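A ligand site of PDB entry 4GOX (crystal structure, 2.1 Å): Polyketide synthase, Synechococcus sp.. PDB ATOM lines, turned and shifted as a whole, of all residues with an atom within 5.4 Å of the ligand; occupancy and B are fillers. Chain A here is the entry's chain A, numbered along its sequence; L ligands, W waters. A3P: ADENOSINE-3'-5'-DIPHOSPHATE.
The side-chain hydroxyl of Ser 37 is in hydrogen-bond range of the side-chain amino group of Lys 128 (3.3 Å). The side-chain hydroxyl (OG) of Ser 164 lies within hydrogen-bond range of the guanidinium group (NE) of Arg 34 (3.0 Å). The side-chain hydroxyl (OH) of Tyr 243 sits at hydrogen-bond distance from the backbone carbonyl oxygen (O) of Phe 264 (2.8 Å). OG1 of Thr 38 is in hydrogen-bond range of N of Asp 261 (2.9 Å). The side-chain hydroxyl of Thr 38 sits at hydrogen-bond distance from the side-chain amino group of Lys 128, at 2.9 Å. O of Arg 34 sits at hydrogen-bond distance from NH1 of Arg 156, 3.0 Å away. The side-chain carboxylate of Asp 261 is in salt-bridge range of the guanidinium group of Arg 34 (3.0 Å). OG of Ser 35 lies within hydrogen-bond range of O of Pro 33, 3.3 Å away.
CD1 of Leu 39 touches N6 of the ligand, at 3.5 Å. CD2 of Leu 168 touches O1P of the ligand (3.8 Å). CG1 of Val 217 touches C2 of the ligand, at 3.7 Å. OD2 of Asp 261 touches C8 of the ligand, 3.4 Å away. CD1 of Phe 264 touches N7 of the ligand, at 3.6 Å. CD2 of His 267 touches N7 of the ligand, at 3.4 Å. CA of Ile 270 touches N1 of the ligand, at 3.7 Å. CD1 of Leu 274 touches N3 of the ligand, at 3.4 Å. 21 residues have an atom within 4 Å of the ligand: Arg 34, Ser 35, Gly 36, Ser 37, Thr 38, Leu 39, Arg 156, Ser 164, Arg 167, Leu 168, Tyr 213, Val 217, Tyr 243, Asp 261, Asn 263, Phe 264, His 267, Thr 269, Ile 270, Asp 271 and Leu 274. Along chain A the residues within 4 Å of the ligand span positions 34 to 274. The nearest printed residue that does not touch the ligand is Pro 33 (4.2 Å).
Water W3 lies within hydrogen-bond range of a ring nitrogen (NE2) of His 267 (2.6 Å), an oxygen (O2P) of the ligand (2.6 Å) and the side-chain carboxylate of Asp 261 (2.6 Å). Water W1 lies within hydrogen-bond range of O6P of the ligand (2.6 Å), N of Leu 39 (2.9 Å) and N of Thr 38 (3.3 Å). Water W2 lies within hydrogen-bond range of NZ of Lys 128 (3.0 Å), OG1 of Thr 38 (3.1 Å) and O5P of the ligand (3.2 Å).
O4P of the ligand sits at hydrogen-bond distance from N of Ser 37, 2.9 Å away. OG of Ser 37 sits at hydrogen-bond distance from O4P of the ligand, at 2.5 Å. The side-chain hydroxyl (OG) of Ser 164 sits at hydrogen-bond distance from an oxygen (O1P) of the ligand, at 2.7 Å. The side-chain hydroxyl (OH) of Tyr 243 lies within hydrogen-bond range of a nitrogen (N6) of the ligand, 2.7 Å away. The side-chain hydroxyl of Tyr 213 is in hydrogen-bond range of a nitrogen (N3) of the ligand. The backbone NH (N) of Thr 38 sits at hydrogen-bond distance from an oxygen (O6P) of the ligand (2.9 Å). OG1 of Thr 38 sits at hydrogen-bond distance from O6P of the ligand, 2.8 Å away. O5P of the ligand is in hydrogen-bond range of N of Arg 34. The guanidinium group (NH2) of Arg 34 lies within salt-bridge range of an oxygen (O5P) of the ligand (2.9 Å). An oxygen (O5') of the ligand sits at hydrogen-bond distance from the backbone NH of Gly 36, 2.9 Å away. O of Thr 269 is in hydrogen-bond range of N6 of the ligand, 2.9 Å away. N of Asp 271 is in hydrogen-bond range of N1 of the ligand (2.9 Å). NH1 of Arg 156 sits at hydrogen-bond distance from O2' of the ligand. NH1 of Arg 167 is in salt-bridge range of O1P of the ligand (3.0 Å). O4P of the ligand is in hydrogen-bond range of N of Ser 35, 3.1 Å away. The side-chain amide nitrogen (ND2) of Asn 263 sits at hydrogen-bond distance from an oxygen (O2P) of the ligand (3.4 Å).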
ATOM      1  N   SER A  31       7.623  -7.186  -7.626  1.00  0.00           N
ATOM      2  CA  SER A  31       8.354  -7.437  -6.385  1.00  0.00           C
ATOM      3  C   SER A  31       7.632  -8.476  -5.572  1.00  0.00           C
ATOM      4  O   SER A  31       6.502  -8.871  -5.871  1.00  0.00           O
ATOM      5  CB  SER A  31       8.467  -6.162  -5.550  1.00  0.00           C
ATOM      6  OG  SER A  31       7.216  -5.778  -4.982  1.00  0.00           O
ATOM      7  N   SER A  32       8.278  -8.868  -4.490  1.00  0.00           N
ATOM      8  CA  SER A  32       7.707  -9.656  -3.432  1.00  0.00           C
ATOM      9  C   SER A  32       6.802  -8.636  -2.667  1.00  0.00           C
ATOM     10  O   SER A  32       7.075  -7.422  -2.734  1.00  0.00           O
ATOM     11  CB  SER A  32       8.845 -10.118  -2.517  1.00  0.00           C
ATOM     12  OG  SER A  32       8.479 -10.294  -1.161  1.00  0.00           O
ATOM     13  N   PRO A  33       5.780  -9.052  -1.888  1.00  0.00           N
ATOM     14  CA  PRO A  33       5.039  -8.048  -1.091  1.00  0.00           C
ATOM     15  C   PRO A  33       5.961  -7.423  -0.032  1.00  0.00           C
ATOM     16  O   PRO A  33       7.027  -7.965   0.269  1.00  0.00           O
ATOM     17  CB  PRO A  33       3.899  -8.846  -0.419  1.00  0.00           C
ATOM     18  CG  PRO A  33       4.193 -10.247  -0.639  1.00  0.00           C
ATOM     19  CD  PRO A  33       5.244 -10.408  -1.703  1.00  0.00           C
ATOM     20  N   ARG A  34       5.545  -6.271   0.538  1.00  0.00           N
ATOM     21  CA  ARG A  34       6.259  -5.560   1.629  1.00  0.00           C
ATOM     22  C   ARG A  34       7.651  -5.039   1.257  1.00  0.00           C
ATOM     23  O   ARG A  34       8.534  -4.975   2.106  1.00  0.00           O
ATOM     24  CB  ARG A  34       6.296  -6.439   2.917  1.00  0.00           C
ATOM     25  CG  ARG A  34       4.961  -7.101   3.325  1.00  0.00           C
ATOM     26  CD  ARG A  34       3.735  -6.195   3.207  1.00  0.00           C
ATOM     27  NE  ARG A  34       3.729  -5.096   4.174  1.00  0.00           N
ATOM     28  CZ  ARG A  34       2.978  -4.001   4.069  1.00  0.00           C
ATOM     29  NH1 ARG A  34       3.012  -3.083   5.020  1.00  0.00           N
ATOM     30  NH2 ARG A  34       2.203  -3.814   3.003  1.00  0.00           N
ATOM     31  N   SER A  35       7.807  -4.657  -0.008  1.00  0.00           N
ATOM     32  CA  SER A  35       9.093  -4.245  -0.600  1.00  0.00           C
ATOM     33  C   SER A  35       9.182  -2.795  -1.046  1.00  0.00           C
ATOM     34  O   SER A  35      10.170  -2.423  -1.680  1.00  0.00           O
ATOM     35  CB  SER A  35       9.440  -5.184  -1.763  1.00  0.00           C
ATOM     36  OG  SER A  35       9.586  -6.519  -1.305  1.00  0.00           O
ATOM     37  N   GLY A  36       8.194  -1.974  -0.684  1.00  0.00           N
ATOM     38  CA  GLY A  36       8.158  -0.569  -1.067  1.00  0.00           C
ATOM     39  C   GLY A  36       7.512  -0.354  -2.420  1.00  0.00           C
ATOM     40  O   GLY A  36       7.669   0.700  -3.034  1.00  0.00           O
ATOM     41  N   SER A  37       6.735  -1.358  -2.880  1.00  0.00           N
ATOM     42  CA  SER A  37       6.105  -1.278  -4.199  1.00  0.00           C
ATOM     43  C   SER A  37       5.015  -0.193  -4.261  1.00  0.00           C
ATOM     44  O   SER A  37       4.926   0.502  -5.276  1.00  0.00           O
ATOM     45  CB  SER A  37       5.592  -2.634  -4.662  1.00  0.00           C
ATOM     46  OG  SER A  37       4.611  -3.132  -3.775  1.00  0.00           O
ATOM     47  N   THR A  38       4.243   0.005  -3.177  1.00  0.00           N
ATOM     48  CA  THR A  38       3.199   1.092  -3.148  1.00  0.00           C
ATOM     49  C   THR A  38       3.886   2.455  -3.192  1.00  0.00           C
ATOM     50  O   THR A  38       3.457   3.307  -3.955  1.00  0.00           O
ATOM     51  CB  THR A  38       2.233   0.937  -1.944  1.00  0.00           C
ATOM     52  OG1 THR A  38       1.744  -0.412  -1.956  1.00  0.00           O
ATOM     53  CG2 THR A  38       1.034   1.909  -1.992  1.00  0.00           C
ATOM     54  N   LEU A  39       4.980   2.637  -2.416  1.00  0.00           N
ATOM     55  CA  LEU A  39       5.780   3.865  -2.404  1.00  0.00           C
ATOM     56  C   LEU A  39       6.325   4.133  -3.811  1.00  0.00           C
ATOM     57  O   LEU A  39       6.136   5.223  -4.327  1.00  0.00           O
ATOM     58  CB  LEU A  39       6.946   3.774  -1.390  1.00  0.00           C
ATOM     59  CG  LEU A  39       7.941   4.960  -1.397  1.00  0.00           C
ATOM     60  CD1 LEU A  39       7.358   6.182  -0.771  1.00  0.00           C
ATOM     61  CD2 LEU A  39       9.245   4.566  -0.741  1.00  0.00           C
ATOM     62  N   LYS A 128       1.685  -2.070 -11.346  1.00  0.00           N
ATOM     63  CA  LYS A 128       2.450  -2.519 -10.188  1.00  0.00           C
ATOM     64  C   LYS A 128       1.766  -3.739  -9.613  1.00  0.00           C
ATOM     65  O   LYS A 128       0.528  -3.732  -9.445  1.00  0.00           O
ATOM     66  CB  LYS A 128       2.517  -1.412  -9.097  1.00  0.00           C
ATOM     67  CG  LYS A 128       3.352  -1.806  -7.857  1.00  0.00           C
ATOM     68  CD  LYS A 128       2.547  -2.452  -6.708  1.00  0.00           C
ATOM     69  CE  LYS A 128       1.924  -1.419  -5.791  1.00  0.00           C
ATOM     70  NZ  LYS A 128       1.610  -1.976  -4.443  1.00  0.00           N
ATOM     71  N   PRO A 130       2.634  -6.787  -6.394  1.00  0.00           N
ATOM     72  CA  PRO A 130       3.501  -7.578  -5.486  1.00  0.00           C
ATOM     73  C   PRO A 130       3.176  -9.087  -5.500  1.00  0.00           C
ATOM     74  O   PRO A 130       3.643  -9.834  -4.653  1.00  0.00           O
ATOM     75  CB  PRO A 130       3.193  -6.981  -4.112  1.00  0.00           C
ATOM     76  CG  PRO A 130       1.771  -6.438  -4.228  1.00  0.00           C
ATOM     77  CD  PRO A 130       1.424  -6.289  -5.709  1.00  0.00           C
ATOM     78  N   ARG A 156      13.860  -5.801  -1.880  1.00  0.00           N
ATOM     79  CA  ARG A 156      14.084  -5.397  -0.477  1.00  0.00           C
ATOM     80  C   ARG A 156      14.759  -6.538   0.262  1.00  0.00           C
ATOM     81  O   ARG A 156      14.640  -7.700  -0.158  1.00  0.00           O
ATOM     82  CB  ARG A 156      12.779  -4.950   0.211  1.00  0.00           C
ATOM     83  CG  ARG A 156      13.021  -4.277   1.578  1.00  0.00           C
ATOM     84  CD  ARG A 156      11.724  -3.809   2.183  1.00  0.00           C
ATOM     85  NE  ARG A 156      11.934  -3.049   3.417  1.00  0.00           N
ATOM     86  CZ  ARG A 156      10.967  -2.638   4.218  1.00  0.00           C
ATOM     87  NH1 ARG A 156       9.701  -2.937   3.953  1.00  0.00           N
ATOM     88  NH2 ARG A 156      11.244  -1.940   5.313  1.00  0.00           N
ATOM     89  N   SER A 164       8.077  -7.532   8.187  1.00  0.00           N
ATOM     90  CA  SER A 164       6.886  -6.788   7.766  1.00  0.00           C
ATOM     91  C   SER A 164       5.707  -7.699   7.424  1.00  0.00           C
ATOM     92  O   SER A 164       4.577  -7.417   7.823  1.00  0.00           O
ATOM     93  CB  SER A 164       7.204  -5.895   6.570  1.00  0.00           C
ATOM     94  OG  SER A 164       5.998  -5.393   6.040  1.00  0.00           O
ATOM     95  N   ARG A 167       4.190  -9.140  10.758  1.00  0.00           N
ATOM     96  CA  ARG A 167       3.399  -8.104  11.425  1.00  0.00           C
ATOM     97  C   ARG A 167       2.008  -7.950  10.821  1.00  0.00           C
ATOM     98  O   ARG A 167       1.010  -7.909  11.552  1.00  0.00           O
ATOM     99  CB  ARG A 167       4.129  -6.752  11.338  1.00  0.00           C
ATOM    100  CG  ARG A 167       5.004  -6.418  12.525  1.00  0.00           C
ATOM    101  CD  ARG A 167       5.185  -4.904  12.640  1.00  0.00           C
ATOM    102  NE  ARG A 167       6.278  -4.394  11.807  1.00  0.00           N
ATOM    103  CZ  ARG A 167       6.128  -3.802  10.626  1.00  0.00           C
ATOM    104  NH1 ARG A 167       4.926  -3.649  10.095  1.00  0.00           N
ATOM    105  NH2 ARG A 167       7.192  -3.362   9.956  1.00  0.00           N
ATOM    106  N   LEU A 168       1.935  -7.880   9.475  1.00  0.00           N
ATOM    107  CA  LEU A 168       0.711  -7.677   8.706  1.00  0.00           C
ATOM    108  C   LEU A 168      -0.267  -8.869   8.671  1.00  0.00           C
ATOM    109  O   LEU A 168      -1.366  -8.725   8.140  1.00  0.00           O
ATOM    110  CB  LEU A 168       1.041  -7.131   7.299  1.00  0.00           C
ATOM    111  CG  LEU A 168       1.146  -5.591   7.085  1.00  0.00           C
ATOM    112  CD1 LEU A 168      -0.194  -4.900   7.259  1.00  0.00           C
ATOM    113  CD2 LEU A 168       2.260  -4.950   7.927  1.00  0.00           C
ATOM    114  N   TYR A 213      15.300  -1.289  -2.942  1.00  0.00           N
ATOM    115  CA  TYR A 213      14.478  -0.475  -2.042  1.00  0.00           C
ATOM    116  C   TYR A 213      15.335   0.393  -1.111  1.00  0.00           C
ATOM    117  O   TYR A 213      15.028   1.575  -0.941  1.00  0.00           O
ATOM    118  CB  TYR A 213      13.528  -1.364  -1.218  1.00  0.00           C
ATOM    119  CG  TYR A 213      12.910  -0.641  -0.049  1.00  0.00           C
ATOM    120  CD1 TYR A 213      11.779   0.148  -0.211  1.00  0.00           C
ATOM    121  CD2 TYR A 213      13.479  -0.724   1.229  1.00  0.00           C
ATOM    122  CE1 TYR A 213      11.207   0.826   0.871  1.00  0.00           C
ATOM    123  CE2 TYR A 213      12.928  -0.045   2.303  1.00  0.00           C
ATOM    124  CZ  TYR A 213      11.788   0.719   2.124  1.00  0.00           C
ATOM    125  OH  TYR A 213      11.250   1.380   3.189  1.00  0.00           O
ATOM    126  N   VAL A 217      15.132   4.529  -0.939  1.00  0.00           N
ATOM    127  CA  VAL A 217      14.776   5.371   0.190  1.00  0.00           C
ATOM    128  C   VAL A 217      15.901   6.259   0.692  1.00  0.00           C
ATOM    129  O   VAL A 217      15.640   7.321   1.266  1.00  0.00           O
ATOM    130  CB  VAL A 217      13.972   4.663   1.301  1.00  0.00           C
ATOM    131  CG1 VAL A 217      12.727   3.989   0.730  1.00  0.00           C
ATOM    132  CG2 VAL A 217      14.829   3.689   2.078  1.00  0.00           C
ATOM    133  N   TYR A 243       3.376  12.099  -1.153  1.00  0.00           N
ATOM    134  CA  TYR A 243       2.284  12.512  -0.276  1.00  0.00           C
ATOM    135  C   TYR A 243       1.561  13.800  -0.691  1.00  0.00           C
ATOM    136  O   TYR A 243       0.685  14.258   0.037  1.00  0.00           O
ATOM    137  CB  TYR A 243       2.718  12.460   1.202  1.00  0.00           C
ATOM    138  CG  TYR A 243       3.121  11.065   1.611  1.00  0.00           C
ATOM    139  CD1 TYR A 243       2.174  10.048   1.720  1.00  0.00           C
ATOM    140  CD2 TYR A 243       4.460  10.742   1.839  1.00  0.00           C
ATOM    141  CE1 TYR A 243       2.545   8.749   2.059  1.00  0.00           C
ATOM    142  CE2 TYR A 243       4.845   9.433   2.150  1.00  0.00           C
ATOM    143  CZ  TYR A 243       3.875   8.449   2.282  1.00  0.00           C
ATOM    144  OH  TYR A 243       4.227   7.162   2.626  1.00  0.00           O
ATOM    145  N   GLY A 260      -2.835  -2.259  -2.142  1.00  0.00           N
ATOM    146  CA  GLY A 260      -1.488  -1.800  -1.865  1.00  0.00           C
ATOM    147  C   GLY A 260      -1.185  -1.866  -0.378  1.00  0.00           C
ATOM    148  O   GLY A 260      -1.824  -2.631   0.346  1.00  0.00           O
ATOM    149  N   ASP A 261      -0.223  -1.052   0.085  1.00  0.00           N
ATOM    150  CA  ASP A 261       0.206  -1.032   1.474  1.00  0.00           C
ATOM    151  C   ASP A 261      -0.844  -0.339   2.341  1.00  0.00           C
ATOM    152  O   ASP A 261      -1.143   0.839   2.116  1.00  0.00           O
ATOM    153  CB  ASP A 261       1.585  -0.361   1.592  1.00  0.00           C
ATOM    154  CG  ASP A 261       2.104  -0.078   2.988  1.00  0.00           C
ATOM    155  OD1 ASP A 261       1.595  -0.699   3.963  1.00  0.00           O
ATOM    156  OD2 ASP A 261       3.058   0.699   3.121  1.00  0.00           O
ATOM    157  N   ASN A 263      -0.631   0.674   5.441  1.00  0.00           N
ATOM    158  CA  ASN A 263       0.027   1.657   6.299  1.00  0.00           C
ATOM    159  C   ASN A 263       0.659   2.823   5.497  1.00  0.00           C
ATOM    160  O   ASN A 263       1.338   3.645   6.101  1.00  0.00           O
ATOM    161  CB  ASN A 263       1.128   0.966   7.138  1.00  0.00           C
ATOM    162  CG  ASN A 263       0.726  -0.313   7.848  1.00  0.00           C
ATOM    163  OD1 ASN A 263      -0.393  -0.472   8.348  1.00  0.00           O
ATOM    164  ND2 ASN A 263       1.683  -1.240   7.953  1.00  0.00           N
ATOM    165  N   PHE A 264       0.474   2.867   4.155  1.00  0.00           N
ATOM    166  CA  PHE A 264       1.113   3.888   3.312  1.00  0.00           C
ATOM    167  C   PHE A 264       0.942   5.326   3.740  1.00  0.00           C
ATOM    168  O   PHE A 264       1.931   6.062   3.766  1.00  0.00           O
ATOM    169  CB  PHE A 264       0.830   3.681   1.810  1.00  0.00           C
ATOM    170  CG  PHE A 264       1.571   4.674   0.924  1.00  0.00           C
ATOM    171  CD1 PHE A 264       2.933   4.536   0.671  1.00  0.00           C
ATOM    172  CD2 PHE A 264       0.897   5.734   0.324  1.00  0.00           C
ATOM    173  CE1 PHE A 264       3.611   5.453  -0.125  1.00  0.00           C
ATOM    174  CE2 PHE A 264       1.578   6.626  -0.507  1.00  0.00           C
ATOM    175  CZ  PHE A 264       2.931   6.497  -0.707  1.00  0.00           C
ATOM    176  N   HIS A 267       2.870   7.616   6.816  1.00  0.00           N
ATOM    177  CA  HIS A 267       4.158   8.305   6.674  1.00  0.00           C
ATOM    178  C   HIS A 267       3.997   9.698   6.119  1.00  0.00           C
ATOM    179  O   HIS A 267       3.024   9.976   5.417  1.00  0.00           O
ATOM    180  CB  HIS A 267       5.137   7.509   5.797  1.00  0.00           C
ATOM    181  CG  HIS A 267       5.123   6.050   6.091  1.00  0.00           C
ATOM    182  ND1 HIS A 267       5.821   5.525   7.148  1.00  0.00           N
ATOM    183  CD2 HIS A 267       4.449   5.060   5.469  1.00  0.00           C
ATOM    184  CE1 HIS A 267       5.573   4.226   7.133  1.00  0.00           C
ATOM    185  NE2 HIS A 267       4.757   3.904   6.136  1.00  0.00           N
ATOM    186  N   THR A 269       7.014  11.344   4.783  1.00  0.00           N
ATOM    187  CA  THR A 269       8.043  11.467   3.744  1.00  0.00           C
ATOM    188  C   THR A 269       8.565  10.111   3.272  1.00  0.00           C
ATOM    189  O   THR A 269       8.170   9.067   3.813  1.00  0.00           O
ATOM    190  CB  THR A 269       9.192  12.346   4.282  1.00  0.00           C
ATOM    191  OG1 THR A 269      10.125  12.571   3.207  1.00  0.00           O
ATOM    192  CG2 THR A 269       9.900  11.718   5.485  1.00  0.00           C
ATOM    193  N   ILE A 270       9.502  10.139   2.294  1.00  0.00           N
ATOM    194  CA  ILE A 270      10.270   8.989   1.820  1.00  0.00           C
ATOM    195  C   ILE A 270      11.191   8.778   3.017  1.00  0.00           C
ATOM    196  O   ILE A 270      12.121   9.583   3.240  1.00  0.00           O
ATOM    197  CB  ILE A 270      11.039   9.290   0.499  1.00  0.00           C
ATOM    198  CG1 ILE A 270      10.073   9.693  -0.642  1.00  0.00           C
ATOM    199  CG2 ILE A 270      11.938   8.088   0.099  1.00  0.00           C
ATOM    200  CD1 ILE A 270      10.682  10.563  -1.707  1.00  0.00           C
ATOM    201  N   ASP A 271      10.821   7.826   3.886  1.00  0.00           N
ATOM    202  CA  ASP A 271      11.500   7.580   5.142  1.00  0.00           C
ATOM    203  C   ASP A 271      12.756   6.696   5.001  1.00  0.00           C
ATOM    204  O   ASP A 271      12.619   5.484   4.852  1.00  0.00           O
ATOM    205  CB  ASP A 271      10.508   7.010   6.168  1.00  0.00           C
ATOM    206  CG  ASP A 271      10.975   7.041   7.616  1.00  0.00           C
ATOM    207  OD1 ASP A 271      12.165   7.367   7.857  1.00  0.00           O
ATOM    208  OD2 ASP A 271      10.154   6.738   8.517  1.00  0.00           O
ATOM    209  N   PRO A 272      13.985   7.259   5.129  1.00  0.00           N
ATOM    210  CA  PRO A 272      15.192   6.422   5.022  1.00  0.00           C
ATOM    211  C   PRO A 272      15.411   5.472   6.206  1.00  0.00           C
ATOM    212  O   PRO A 272      16.215   4.557   6.075  1.00  0.00           O
ATOM    213  CB  PRO A 272      16.326   7.447   4.914  1.00  0.00           C
ATOM    214  CG  PRO A 272      15.802   8.662   5.602  1.00  0.00           C
ATOM    215  CD  PRO A 272      14.325   8.683   5.356  1.00  0.00           C
ATOM    216  N   LEU A 274      13.172   3.348   7.426  1.00  0.00           N
ATOM    217  CA  LEU A 274      12.501   2.077   7.110  1.00  0.00           C
ATOM    218  C   LEU A 274      13.396   1.093   6.367  1.00  0.00           C
ATOM    219  O   LEU A 274      13.167  -0.117   6.470  1.00  0.00           O
ATOM    220  CB  LEU A 274      11.146   2.275   6.413  1.00  0.00           C
ATOM    221  CG  LEU A 274      10.082   3.021   7.220  1.00  0.00           C
ATOM    222  CD1 LEU A 274       8.961   3.476   6.347  1.00  0.00           C
ATOM    223  CD2 LEU A 274       9.528   2.189   8.372  1.00  0.00           C
HETATM  224  P1  A3P L   1       5.901  -1.664   6.708  1.00  0.00           P
HETATM  225  O1P A3P L   1       5.481  -3.023   7.196  1.00  0.00           O
HETATM  226  O2P A3P L   1       4.780  -0.654   6.794  1.00  0.00           O
HETATM  227  O3P A3P L   1       7.257  -1.198   7.180  1.00  0.00           O
HETATM  228  P2  A3P L   1       4.565  -2.818  -0.341  1.00  0.00           P
HETATM  229  O4P A3P L   1       5.338  -3.473  -1.446  1.00  0.00           O
HETATM  230  O5P A3P L   1       3.633  -3.690   0.446  1.00  0.00           O
HETATM  231  O6P A3P L   1       3.983  -1.476  -0.752  1.00  0.00           O
HETATM  232  O5' A3P L   1       5.666  -2.395   0.755  1.00  0.00           O
HETATM  233  C5' A3P L   1       5.273  -1.972   2.067  1.00  0.00           C
HETATM  234  C4' A3P L   1       6.482  -1.347   2.767  1.00  0.00           C
HETATM  235  O4' A3P L   1       6.977  -0.211   2.074  1.00  0.00           O
HETATM  236  C3' A3P L   1       6.193  -0.814   4.162  1.00  0.00           C
HETATM  237  O3' A3P L   1       6.171  -1.863   5.116  1.00  0.00           O
HETATM  238  C2' A3P L   1       7.311   0.181   4.368  1.00  0.00           C
HETATM  239  O2' A3P L   1       8.460  -0.414   4.987  1.00  0.00           O
HETATM  240  C1' A3P L   1       7.684   0.635   2.975  1.00  0.00           C
HETATM  241  N9  A3P L   1       7.219   2.040   2.838  1.00  0.00           N
HETATM  242  C8  A3P L   1       5.913   2.432   2.721  1.00  0.00           C
HETATM  243  N7  A3P L   1       5.819   3.779   2.663  1.00  0.00           N
HETATM  244  C5  A3P L   1       7.074   4.256   2.764  1.00  0.00           C
HETATM  245  C6  A3P L   1       7.668   5.606   2.809  1.00  0.00           C
HETATM  246  N6  A3P L   1       6.871   6.675   2.690  1.00  0.00           N
HETATM  247  N1  A3P L   1       9.018   5.703   2.921  1.00  0.00           N
HETATM  248  C2  A3P L   1       9.818   4.609   3.004  1.00  0.00           C
HETATM  249  N3  A3P L   1       9.336   3.352   3.010  1.00  0.00           N
HETATM  250  C4  A3P L   1       7.996   3.119   2.889  1.00  0.00           C
HETATM  251  O   HOH W   1       5.223   0.793  -0.172  1.00  0.00           O
HETATM  252  O   HOH W   2       1.456  -3.514  -1.922  1.00  0.00           O
HETATM  253  O   HOH W   3       4.054   1.483   5.437  1.00  0.00           O
